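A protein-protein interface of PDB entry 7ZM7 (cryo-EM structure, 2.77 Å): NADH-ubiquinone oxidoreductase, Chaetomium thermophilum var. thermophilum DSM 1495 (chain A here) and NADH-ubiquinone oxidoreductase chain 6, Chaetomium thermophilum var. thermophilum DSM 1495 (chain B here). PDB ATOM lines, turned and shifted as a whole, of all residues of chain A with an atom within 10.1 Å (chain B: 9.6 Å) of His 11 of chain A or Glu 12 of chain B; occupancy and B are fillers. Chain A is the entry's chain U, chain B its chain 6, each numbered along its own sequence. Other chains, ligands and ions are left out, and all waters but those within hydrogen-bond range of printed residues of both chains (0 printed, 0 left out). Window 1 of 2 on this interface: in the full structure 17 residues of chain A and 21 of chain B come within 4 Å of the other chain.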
ATOM      1  N   PRO A   6     -20.899  20.012  -4.395  1.00  0.00           N
ATOM      2  CA  PRO A   6     -21.376  21.322  -4.809  1.00  0.00           C
ATOM      3  C   PRO A   6     -22.216  21.299  -6.096  1.00  0.00           C
ATOM      4  O   PRO A   6     -21.932  20.499  -6.956  1.00  0.00           O
ATOM      5  CB  PRO A   6     -20.062  22.092  -4.936  1.00  0.00           C
ATOM      6  CG  PRO A   6     -19.052  21.064  -5.387  1.00  0.00           C
ATOM      7  CD  PRO A   6     -19.540  19.735  -4.851  1.00  0.00           C
ATOM      8  N   ALA A   7     -23.196  22.183  -6.230  1.00  0.00           N
ATOM      9  CA  ALA A   7     -24.107  22.129  -7.395  1.00  0.00           C
ATOM     10  C   ALA A   7     -23.966  23.385  -8.253  1.00  0.00           C
ATOM     11  O   ALA A   7     -24.125  23.279  -9.474  1.00  0.00           O
ATOM     12  CB  ALA A   7     -25.529  21.984  -6.897  1.00  0.00           C
ATOM     13  N   PHE A   8     -23.703  24.525  -7.632  1.00  0.00           N
ATOM     14  CA  PHE A   8     -23.646  25.803  -8.380  1.00  0.00           C
ATOM     15  C   PHE A   8     -22.306  26.495  -8.121  1.00  0.00           C
ATOM     16  O   PHE A   8     -22.286  27.728  -8.069  1.00  0.00           O
ATOM     17  CB  PHE A   8     -24.848  26.678  -8.019  1.00  0.00           C
ATOM     18  CG  PHE A   8     -26.191  26.023  -8.204  1.00  0.00           C
ATOM     19  CD1 PHE A   8     -26.767  25.930  -9.457  1.00  0.00           C
ATOM     20  CD2 PHE A   8     -26.880  25.505  -7.123  1.00  0.00           C
ATOM     21  CE1 PHE A   8     -28.002  25.326  -9.627  1.00  0.00           C
ATOM     22  CE2 PHE A   8     -28.111  24.896  -7.295  1.00  0.00           C
ATOM     23  CZ  PHE A   8     -28.670  24.809  -8.546  1.00  0.00           C
ATOM     24  N   ASN A   9     -21.242  25.726  -7.909  1.00  0.00           N
ATOM     25  CA  ASN A   9     -19.888  26.305  -7.709  1.00  0.00           C
ATOM     26  C   ASN A   9     -19.374  26.916  -9.015  1.00  0.00           C
ATOM     27  O   ASN A   9     -19.446  26.249 -10.044  1.00  0.00           O
ATOM     28  CB  ASN A   9     -18.906  25.271  -7.168  1.00  0.00           C
ATOM     29  CG  ASN A   9     -18.978  23.931  -7.869  1.00  0.00           C
ATOM     30  OD1 ASN A   9     -20.058  23.399  -8.111  1.00  0.00           O
ATOM     31  ND2 ASN A   9     -17.828  23.375  -8.198  1.00  0.00           N
ATOM     32  N   GLN A  10     -18.864  28.146  -8.956  1.00  0.00           N
ATOM     33  CA  GLN A  10     -18.320  28.825 -10.159  1.00  0.00           C
ATOM     34  C   GLN A  10     -16.919  29.375  -9.859  1.00  0.00           C
ATOM     35  O   GLN A  10     -16.227  29.726 -10.820  1.00  0.00           O
ATOM     36  CB  GLN A  10     -19.271  29.934 -10.611  1.00  0.00           C
ATOM     37  CG  GLN A  10     -20.654  29.435 -11.004  1.00  0.00           C
ATOM     38  CD  GLN A  10     -20.634  28.583 -12.248  1.00  0.00           C
ATOM     39  OE1 GLN A  10     -19.948  28.885 -13.220  1.00  0.00           O
ATOM     40  NE2 GLN A  10     -21.401  27.509 -12.230  1.00  0.00           N
ATOM     41  N   HIS A  11     -16.519  29.424  -8.584  1.00  0.00           N
ATOM     42  CA  HIS A  11     -15.207  30.016  -8.192  1.00  0.00           C
ATOM     43  C   HIS A  11     -14.424  29.129  -7.211  1.00  0.00           C
ATOM     44  O   HIS A  11     -15.043  28.277  -6.585  1.00  0.00           O
ATOM     45  CB  HIS A  11     -15.374  31.437  -7.613  1.00  0.00           C
ATOM     46  CG  HIS A  11     -16.019  32.443  -8.501  1.00  0.00           C
ATOM     47  ND1 HIS A  11     -15.402  32.938  -9.628  1.00  0.00           N
ATOM     48  CD2 HIS A  11     -17.197  33.090  -8.400  1.00  0.00           C
ATOM     49  CE1 HIS A  11     -16.185  33.823 -10.203  1.00  0.00           C
ATOM     50  NE2 HIS A  11     -17.293  33.935  -9.467  1.00  0.00           N
ATOM     51  N   VAL A  12     -13.103  29.308  -7.114  1.00  0.00           N
ATOM     52  CA  VAL A  12     -12.240  28.586  -6.186  1.00  0.00           C
ATOM     53  C   VAL A  12     -11.582  29.593  -5.260  1.00  0.00           C
ATOM     54  O   VAL A  12     -11.164  30.664  -5.707  1.00  0.00           O
ATOM     55  CB  VAL A  12     -11.185  27.747  -6.927  1.00  0.00           C
ATOM     56  CG1 VAL A  12     -10.083  27.352  -5.992  1.00  0.00           C
ATOM     57  CG2 VAL A  12     -11.830  26.505  -7.510  1.00  0.00           C
ATOM     58  N   LEU A  13     -11.507  29.266  -3.975  1.00  0.00           N
ATOM     59  CA  LEU A  13     -10.875  30.128  -2.984  1.00  0.00           C
ATOM     60  C   LEU A  13      -9.599  29.479  -2.461  1.00  0.00           C
ATOM     61  O   LEU A  13      -9.656  28.491  -1.727  1.00  0.00           O
ATOM     62  CB  LEU A  13     -11.831  30.436  -1.842  1.00  0.00           C
ATOM     63  CG  LEU A  13     -11.229  31.172  -0.657  1.00  0.00           C
ATOM     64  CD1 LEU A  13     -10.833  32.581  -1.017  1.00  0.00           C
ATOM     65  CD2 LEU A  13     -12.215  31.184   0.451  1.00  0.00           C
ATOM     66  N   LEU A  14      -8.450  30.066  -2.795  1.00  0.00           N
ATOM     67  CA  LEU A  14      -7.119  29.541  -2.400  1.00  0.00           C
ATOM     68  C   LEU A  14      -6.574  30.363  -1.233  1.00  0.00           C
ATOM     69  O   LEU A  14      -6.840  31.559  -1.193  1.00  0.00           O
ATOM     70  CB  LEU A  14      -6.169  29.593  -3.600  1.00  0.00           C
ATOM     71  CG  LEU A  14      -6.359  28.520  -4.668  1.00  0.00           C
ATOM     72  CD1 LEU A  14      -5.115  28.410  -5.531  1.00  0.00           C
ATOM     73  CD2 LEU A  14      -6.666  27.177  -4.035  1.00  0.00           C
ATOM     74  N   LEU B   8      -7.271  34.109  -2.180  1.00  0.00           N
ATOM     75  CA  LEU B   8      -7.253  34.270  -3.655  1.00  0.00           C
ATOM     76  C   LEU B   8      -8.535  33.703  -4.273  1.00  0.00           C
ATOM     77  O   LEU B   8      -8.848  32.545  -4.000  1.00  0.00           O
ATOM     78  CB  LEU B   8      -6.003  33.575  -4.199  1.00  0.00           C
ATOM     79  CG  LEU B   8      -4.701  34.359  -4.056  1.00  0.00           C
ATOM     80  CD1 LEU B   8      -3.613  33.728  -4.907  1.00  0.00           C
ATOM     81  CD2 LEU B   8      -4.901  35.810  -4.459  1.00  0.00           C
ATOM     82  N   LEU B   9      -9.276  34.438  -5.013  1.00  0.00           N
ATOM     83  CA  LEU B   9     -10.549  33.969  -5.613  1.00  0.00           C
ATOM     84  C   LEU B   9     -10.388  33.942  -7.133  1.00  0.00           C
ATOM     85  O   LEU B   9     -10.037  34.991  -7.698  1.00  0.00           O
ATOM     86  CB  LEU B   9     -11.654  34.950  -5.212  1.00  0.00           C
ATOM     87  CG  LEU B   9     -13.084  34.498  -5.497  1.00  0.00           C
ATOM     88  CD1 LEU B   9     -13.390  33.195  -4.776  1.00  0.00           C
ATOM     89  CD2 LEU B   9     -14.074  35.574  -5.082  1.00  0.00           C
ATOM     90  N   LEU B  10     -10.606  32.848  -7.763  1.00  0.00           N
ATOM     91  CA  LEU B  10     -10.540  32.701  -9.207  1.00  0.00           C
ATOM     92  C   LEU B  10     -11.647  31.785  -9.701  1.00  0.00           C
ATOM     93  O   LEU B  10     -12.153  30.927  -8.978  1.00  0.00           O
ATOM     94  CB  LEU B  10      -9.185  32.179  -9.679  1.00  0.00           C
ATOM     95  CG  LEU B  10      -8.754  30.738  -9.472  1.00  0.00           C
ATOM     96  CD1 LEU B  10      -7.586  30.446 -10.379  1.00  0.00           C
ATOM     97  CD2 LEU B  10      -8.327  30.567  -8.055  1.00  0.00           C
ATOM     98  N   LYS B  11     -11.996  31.892 -10.989  1.00  0.00           N
ATOM     99  CA  LYS B  11     -13.101  31.075 -11.580  1.00  0.00           C
ATOM    100  C   LYS B  11     -12.697  29.599 -11.738  1.00  0.00           C
ATOM    101  O   LYS B  11     -11.494  29.305 -11.618  1.00  0.00           O
ATOM    102  CB  LYS B  11     -13.478  31.669 -12.942  1.00  0.00           C
ATOM    103  CG  LYS B  11     -14.796  31.200 -13.545  1.00  0.00           C
ATOM    104  CD  LYS B  11     -14.844  31.376 -15.045  1.00  0.00           C
ATOM    105  CE  LYS B  11     -16.050  30.717 -15.679  1.00  0.00           C
ATOM    106  NZ  LYS B  11     -16.058  30.887 -17.151  1.00  0.00           N
ATOM    107  N   GLU B  12     -13.661  28.704 -11.996  1.00  0.00           N
ATOM    108  CA  GLU B  12     -13.354  27.264 -12.247  1.00  0.00           C
ATOM    109  C   GLU B  12     -13.486  26.992 -13.749  1.00  0.00           C
ATOM    110  O   GLU B  12     -14.590  27.205 -14.286  1.00  0.00           O
ATOM    111  CB  GLU B  12     -14.318  26.361 -11.481  1.00  0.00           C
ATOM    112  CG  GLU B  12     -14.381  26.650  -9.995  1.00  0.00           C
ATOM    113  CD  GLU B  12     -15.457  25.868  -9.262  1.00  0.00           C
ATOM    114  OE1 GLU B  12     -16.265  25.211  -9.935  1.00  0.00           O
ATOM    115  OE2 GLU B  12     -15.481  25.916  -8.023  1.00  0.00           O
ATOM    116  N   ILE B  13     -12.405  26.562 -14.404  1.00  0.00           N
ATOM    117  CA  ILE B  13     -12.403  26.380 -15.891  1.00  0.00           C
ATOM    118  C   ILE B  13     -13.250  25.205 -16.426  1.00  0.00           C
ATOM    119  O   ILE B  13     -13.980  25.441 -17.413  1.00  0.00           O
ATOM    120  CB  ILE B  13     -10.953  26.404 -16.424  1.00  0.00           C
ATOM    121  CG1 ILE B  13     -10.889  26.367 -17.954  1.00  0.00           C
ATOM    122  CG2 ILE B  13     -10.109  25.313 -15.784  1.00  0.00           C
ATOM    123  CD1 ILE B  13     -11.469  27.590 -18.624  1.00  0.00           C
ATOM    124  N   TYR B  14     -13.211  24.006 -15.826  1.00  0.00           N
ATOM    125  CA  TYR B  14     -13.919  22.843 -16.446  1.00  0.00           C
ATOM    126  C   TYR B  14     -14.846  22.145 -15.451  1.00  0.00           C
ATOM    127  O   TYR B  14     -16.014  21.936 -15.798  1.00  0.00           O
ATOM    128  CB  TYR B  14     -12.927  21.857 -17.067  1.00  0.00           C
ATOM    129  CG  TYR B  14     -12.220  22.369 -18.296  1.00  0.00           C
ATOM    130  CD1 TYR B  14     -10.866  22.652 -18.276  1.00  0.00           C
ATOM    131  CD2 TYR B  14     -12.907  22.580 -19.481  1.00  0.00           C
ATOM    132  CE1 TYR B  14     -10.211  23.126 -19.399  1.00  0.00           C
ATOM    133  CE2 TYR B  14     -12.267  23.054 -20.613  1.00  0.00           C
ATOM    134  CZ  TYR B  14     -10.913  23.328 -20.572  1.00  0.00           C
ATOM    135  OH  TYR B  14     -10.268  23.795 -21.682  1.00  0.00           O
ATOM    136  N   THR B  15     -14.320  21.682 -14.319  1.00  0.00           N
ATOM    137  CA  THR B  15     -15.204  21.159 -13.242  1.00  0.00           C
ATOM    138  C   THR B  15     -15.933  22.324 -12.578  1.00  0.00           C
ATOM    139  O   THR B  15     -15.629  22.602 -11.415  1.00  0.00           O
ATOM    140  CB  THR B  15     -14.423  20.311 -12.232  1.00  0.00           C
ATOM    141  OG1 THR B  15     -13.477  21.137 -11.554  1.00  0.00           O
ATOM    142  CG2 THR B  15     -13.718  19.138 -12.874  1.00  0.00           C
ATOM    143  N   ASN B  16     -16.887  22.941 -13.272  1.00  0.00           N
ATOM    144  CA  ASN B  16     -17.528  24.158 -12.706  1.00  0.00           C
ATOM    145  C   ASN B  16     -18.821  23.815 -11.967  1.00  0.00           C
ATOM    146  O   ASN B  16     -18.734  23.557 -10.765  1.00  0.00           O
ATOM    147  CB  ASN B  16     -17.675  25.299 -13.721  1.00  0.00           C
ATOM    148  CG  ASN B  16     -18.275  24.883 -15.048  1.00  0.00           C
ATOM    149  OD1 ASN B  16     -17.819  23.931 -15.676  1.00  0.00           O
ATOM    150  ND2 ASN B  16     -19.290  25.607 -15.492  1.00  0.00           N
ATOM    151  N   GLY B  17     -19.957  23.755 -12.656  1.00  0.00           N
ATOM    152  CA  GLY B  17     -21.250  23.599 -11.969  1.00  0.00           C
ATOM    153  C   GLY B  17     -22.314  24.354 -12.728  1.00  0.00           C
ATOM    154  O   GLY B  17     -22.109  24.601 -13.925  1.00  0.00           O
ATOM    155  N   SER B  18     -23.418  24.682 -12.070  1.00  0.00           N
ATOM    156  CA  SER B  18     -24.530  25.367 -12.765  1.00  0.00           C
ATOM    157  C   SER B  18     -24.635  26.801 -12.265  1.00  0.00           C
ATOM    158  O   SER B  18     -24.072  27.095 -11.210  1.00  0.00           O
ATOM    159  CB  SER B  18     -25.822  24.640 -12.558  1.00  0.00           C
ATOM    160  OG  SER B  18     -25.730  23.300 -13.016  1.00  0.00           O
ATOM    161  N   THR B  19     -25.279  27.676 -13.029  1.00  0.00           N
ATOM    162  CA  THR B  19     -25.537  29.049 -12.529  1.00  0.00           C
ATOM    163  C   THR B  19     -26.625  28.991 -11.452  1.00  0.00           C
ATOM    164  O   THR B  19     -27.541  28.160 -11.581  1.00  0.00           O
ATOM    165  CB  THR B  19     -25.791  30.030 -13.677  1.00  0.00           C
ATOM    166  OG1 THR B  19     -25.691  31.350 -13.149  1.00  0.00           O
ATOM    167  CG2 THR B  19     -27.122  29.836 -14.366  1.00  0.00           C
ATOM    168  N   HIS B  20     -26.537  29.839 -10.437  1.00  0.00           N
ATOM    169  CA  HIS B  20     -27.624  29.876  -9.437  1.00  0.00           C
ATOM    170  C   HIS B  20     -28.755  30.728 -10.001  1.00  0.00           C
ATOM    171  O   HIS B  20     -29.831  30.779  -9.382  1.00  0.00           O
ATOM    172  CB  HIS B  20     -27.107  30.470  -8.121  1.00  0.00           C
ATOM    173  CG  HIS B  20     -26.515  31.830  -8.266  1.00  0.00           C
ATOM    174  ND1 HIS B  20     -25.183  32.025  -8.572  1.00  0.00           N
ATOM    175  CD2 HIS B  20     -27.061  33.059  -8.147  1.00  0.00           C
ATOM    176  CE1 HIS B  20     -24.935  33.316  -8.639  1.00  0.00           C
ATOM    177  NE2 HIS B  20     -26.071  33.972  -8.381  1.00  0.00           N
ATOM    178  N   PHE B 168     -20.566  33.472   1.145  1.00  0.00           N
ATOM    179  CA  PHE B 168     -20.368  32.371   0.225  1.00  0.00           C
ATOM    180  C   PHE B 168     -20.258  31.074   1.003  1.00  0.00           C
ATOM    181  O   PHE B 168     -19.588  31.005   2.031  1.00  0.00           O
ATOM    182  CB  PHE B 168     -19.107  32.575  -0.613  1.00  0.00           C
ATOM    183  CG  PHE B 168     -19.313  33.416  -1.826  1.00  0.00           C
ATOM    184  CD1 PHE B 168     -19.696  32.841  -3.020  1.00  0.00           C
ATOM    185  CD2 PHE B 168     -19.069  34.774  -1.791  1.00  0.00           C
ATOM    186  CE1 PHE B 168     -19.874  33.605  -4.137  1.00  0.00           C
ATOM    187  CE2 PHE B 168     -19.241  35.540  -2.905  1.00  0.00           C
ATOM    188  CZ  PHE B 168     -19.644  34.955  -4.083  1.00  0.00           C
ATOM    189  N   PHE B 169     -20.898  30.032   0.468  1.00  0.00           N
ATOM    190  CA  PHE B 169     -20.770  28.676   1.058  1.00  0.00           C
ATOM    191  C   PHE B 169     -19.468  28.077   0.530  1.00  0.00           C
ATOM    192  O   PHE B 169     -19.127  28.326  -0.629  1.00  0.00           O
ATOM    193  CB  PHE B 169     -21.934  27.791   0.610  1.00  0.00           C
ATOM    194  CG  PHE B 169     -23.230  28.033   1.336  1.00  0.00           C
ATOM    195  CD1 PHE B 169     -23.445  27.497   2.595  1.00  0.00           C
ATOM    196  CD2 PHE B 169     -24.238  28.782   0.756  1.00  0.00           C
ATOM    197  CE1 PHE B 169     -24.640  27.708   3.261  1.00  0.00           C
ATOM    198  CE2 PHE B 169     -25.432  28.995   1.424  1.00  0.00           C
ATOM    199  CZ  PHE B 169     -25.630  28.456   2.672  1.00  0.00           C
ATOM    200  N   ILE B 170     -18.757  27.326   1.364  1.00  0.00           N
ATOM    201  CA  ILE B 170     -17.443  26.754   0.953  1.00  0.00           C
ATOM    202  C   ILE B 170     -17.511  25.231   1.054  1.00  0.00           C
ATOM    203  O   ILE B 170     -18.172  24.740   1.981  1.00  0.00           O
ATOM    204  CB  ILE B 170     -16.281  27.361   1.774  1.00  0.00           C
ATOM    205  CG1 ILE B 170     -14.907  26.942   1.243  1.00  0.00           C
ATOM    206  CG2 ILE B 170     -16.424  27.079   3.261  1.00  0.00           C
ATOM    207  CD1 ILE B 170     -14.264  27.959   0.344  1.00  0.00           C
ATOM    208  N   THR B 171     -16.892  24.521   0.110  1.00  0.00           N
ATOM    209  CA  THR B 171     -16.830  23.040   0.192  1.00  0.00           C
ATOM    210  C   THR B 171     -15.411  22.537  -0.083  1.00  0.00           C
ATOM    211  O   THR B 171     -14.689  23.211  -0.826  1.00  0.00           O
ATOM    212  CB  THR B 171     -17.856  22.355  -0.718  1.00  0.00           C
ATOM    213  OG1 THR B 171     -17.881  23.013  -1.984  1.00  0.00           O
ATOM    214  CG2 THR B 171     -19.239  22.306  -0.109  1.00  0.00           C
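The backbone carbonyl oxygen (O) of Leu 14 of chain A lies within hydrogen-bond range of the backbone NH (N) of Leu 8 of chain B. The side-chain carboxylate (OE2) of Glu 12 of chain B sits close to the backbone carbonyl oxygen (O) of His 11 of chain A, at 2.8 Å. The side-chain amide nitrogen (NE2) of Gln 10 of chain A sits at hydrogen-bond distance from the backbone carbonyl oxygen (O) of Ser 18 of chain B. NE2 of Gln 10 of chain A lies close to O of Gly 17 of chain B. The backbone NH (N) of Val 12 of chain A sits at hydrogen-bond distance from the backbone carbonyl oxygen (O) of Leu 10 of chain B (2.6 Å). ND2 of Asn 9 of chain A lies within hydrogen-bond range of OE1 of Glu 12 of chain B (3.0 Å). The backbone carbonyl oxygen (O) of Val 12 of chain A sits close to the backbone carbonyl oxygen (O) of Leu 8 of chain B (3.4 Å). The backbone carbonyl oxygen (O) of Gln 10 of chain A sits at hydrogen-bond distance from the backbone NH (N) of Glu 12 of chain B. O of Ala 7 of chain A is in hydrogen-bond range of N of Ser 18 of chain B (3.0 Å). ND2 of Asn 9 of chain A lies within hydrogen-bond range of O of Asn 16 of chain B (2.7 Å).
The side-chain amide oxygen (OD1) of Asn 16 of chain B sits close to the backbone carbonyl oxygen (O) of Tyr 14 of chain B (2.7 Å).
Among the printed residues, pairs that only touch across the chains: Phe 8 of chain A with Ser 18 of chain B (3.1 Å), Phe 8 of chain A with Thr 19 of chain B (3.2 Å), His 11 of chain A with Leu 10 of chain B (3.3 Å), Leu 13 of chain A with Leu 8 of chain B (3.3 Å), Val 12 of chain A with Leu 9 of chain B (3.4 Å), Gln 10 of chain A with Lys 11 of chain B (3.4 Å), His 11 of chain A with Lys 11 of chain B (3.5 Å), Val 12 of chain A with Glu 12 of chain B (3.6 Å), Asn 9 of chain A with Gly 17 of chain B (3.6 Å), Pro 6 of chain A with Thr 171 of chain B (3.8 Å), Ala 7 of chain A with Gly 17 of chain B (3.8 Å), Leu 13 of chain A with Ile 170 of chain B (3.8 Å), His 11 of chain A with Leu 9 of chain B (3.9 Å), Gln 10 of chain A with Thr 19 of chain B (3.96 Å) and Asn 9 of chain A with Thr 15 of chain B (3.97 Å).
Of the printed residues of chain B, Pro 6 of chain A touches Thr 171 (3.8 Å). Printed residues of chain B within 4 Å of Ala 7 of chain A: Gly 17 (3.8 Å) and Ser 18 (3.0 Å). Printed residues of chain B within 4 Å of Phe 8 of chain A: Ser 18 and Thr 19. Asn 9 of chain A touches just these residues of chain B: Glu 12, Thr 15, Asn 16 and Gly 17. Of chain B, only Leu 9, Leu 10, Lys 11 and Glu 12 come within 4 Å of His 11 of chain A. Of chain B, only Leu 8 (3.4 Å), Leu 9 (3.4 Å), Leu 10 (2.6 Å) and Glu 12 (3.6 Å) come within 4 Å of Val 12 of chain A. No residue of chain A comes within 4 Å of Ile 13 of chain B. Phe 168 of chain B touches none of the printed residues of chain A. Phe 169 of chain B touches none of the printed residues of chain A. The nearest residue of chain B that does not touch His 11 of chain A is Phe 168 of chain B (5.1 Å). The nearest residue of chain A that does not touch Glu 12 of chain B is Phe 8 of chain A (6.4 Å). The nearest printed residue of chain A that does not touch Leu 9 of chain B is Leu 13 of chain A (4.3 Å).
Hydrophobic or aromatic side chains of chain B within 4 Å of the printed part of chain A: Leu 8, Leu 9, Leu 10 and Ile 170. Among the printed residues, 25 pairs touch across the chains. Among the printed residues, no Asp or Glu carboxylate lies within 4 Å of a Lys or Arg side-chain nitrogen of the other chain.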
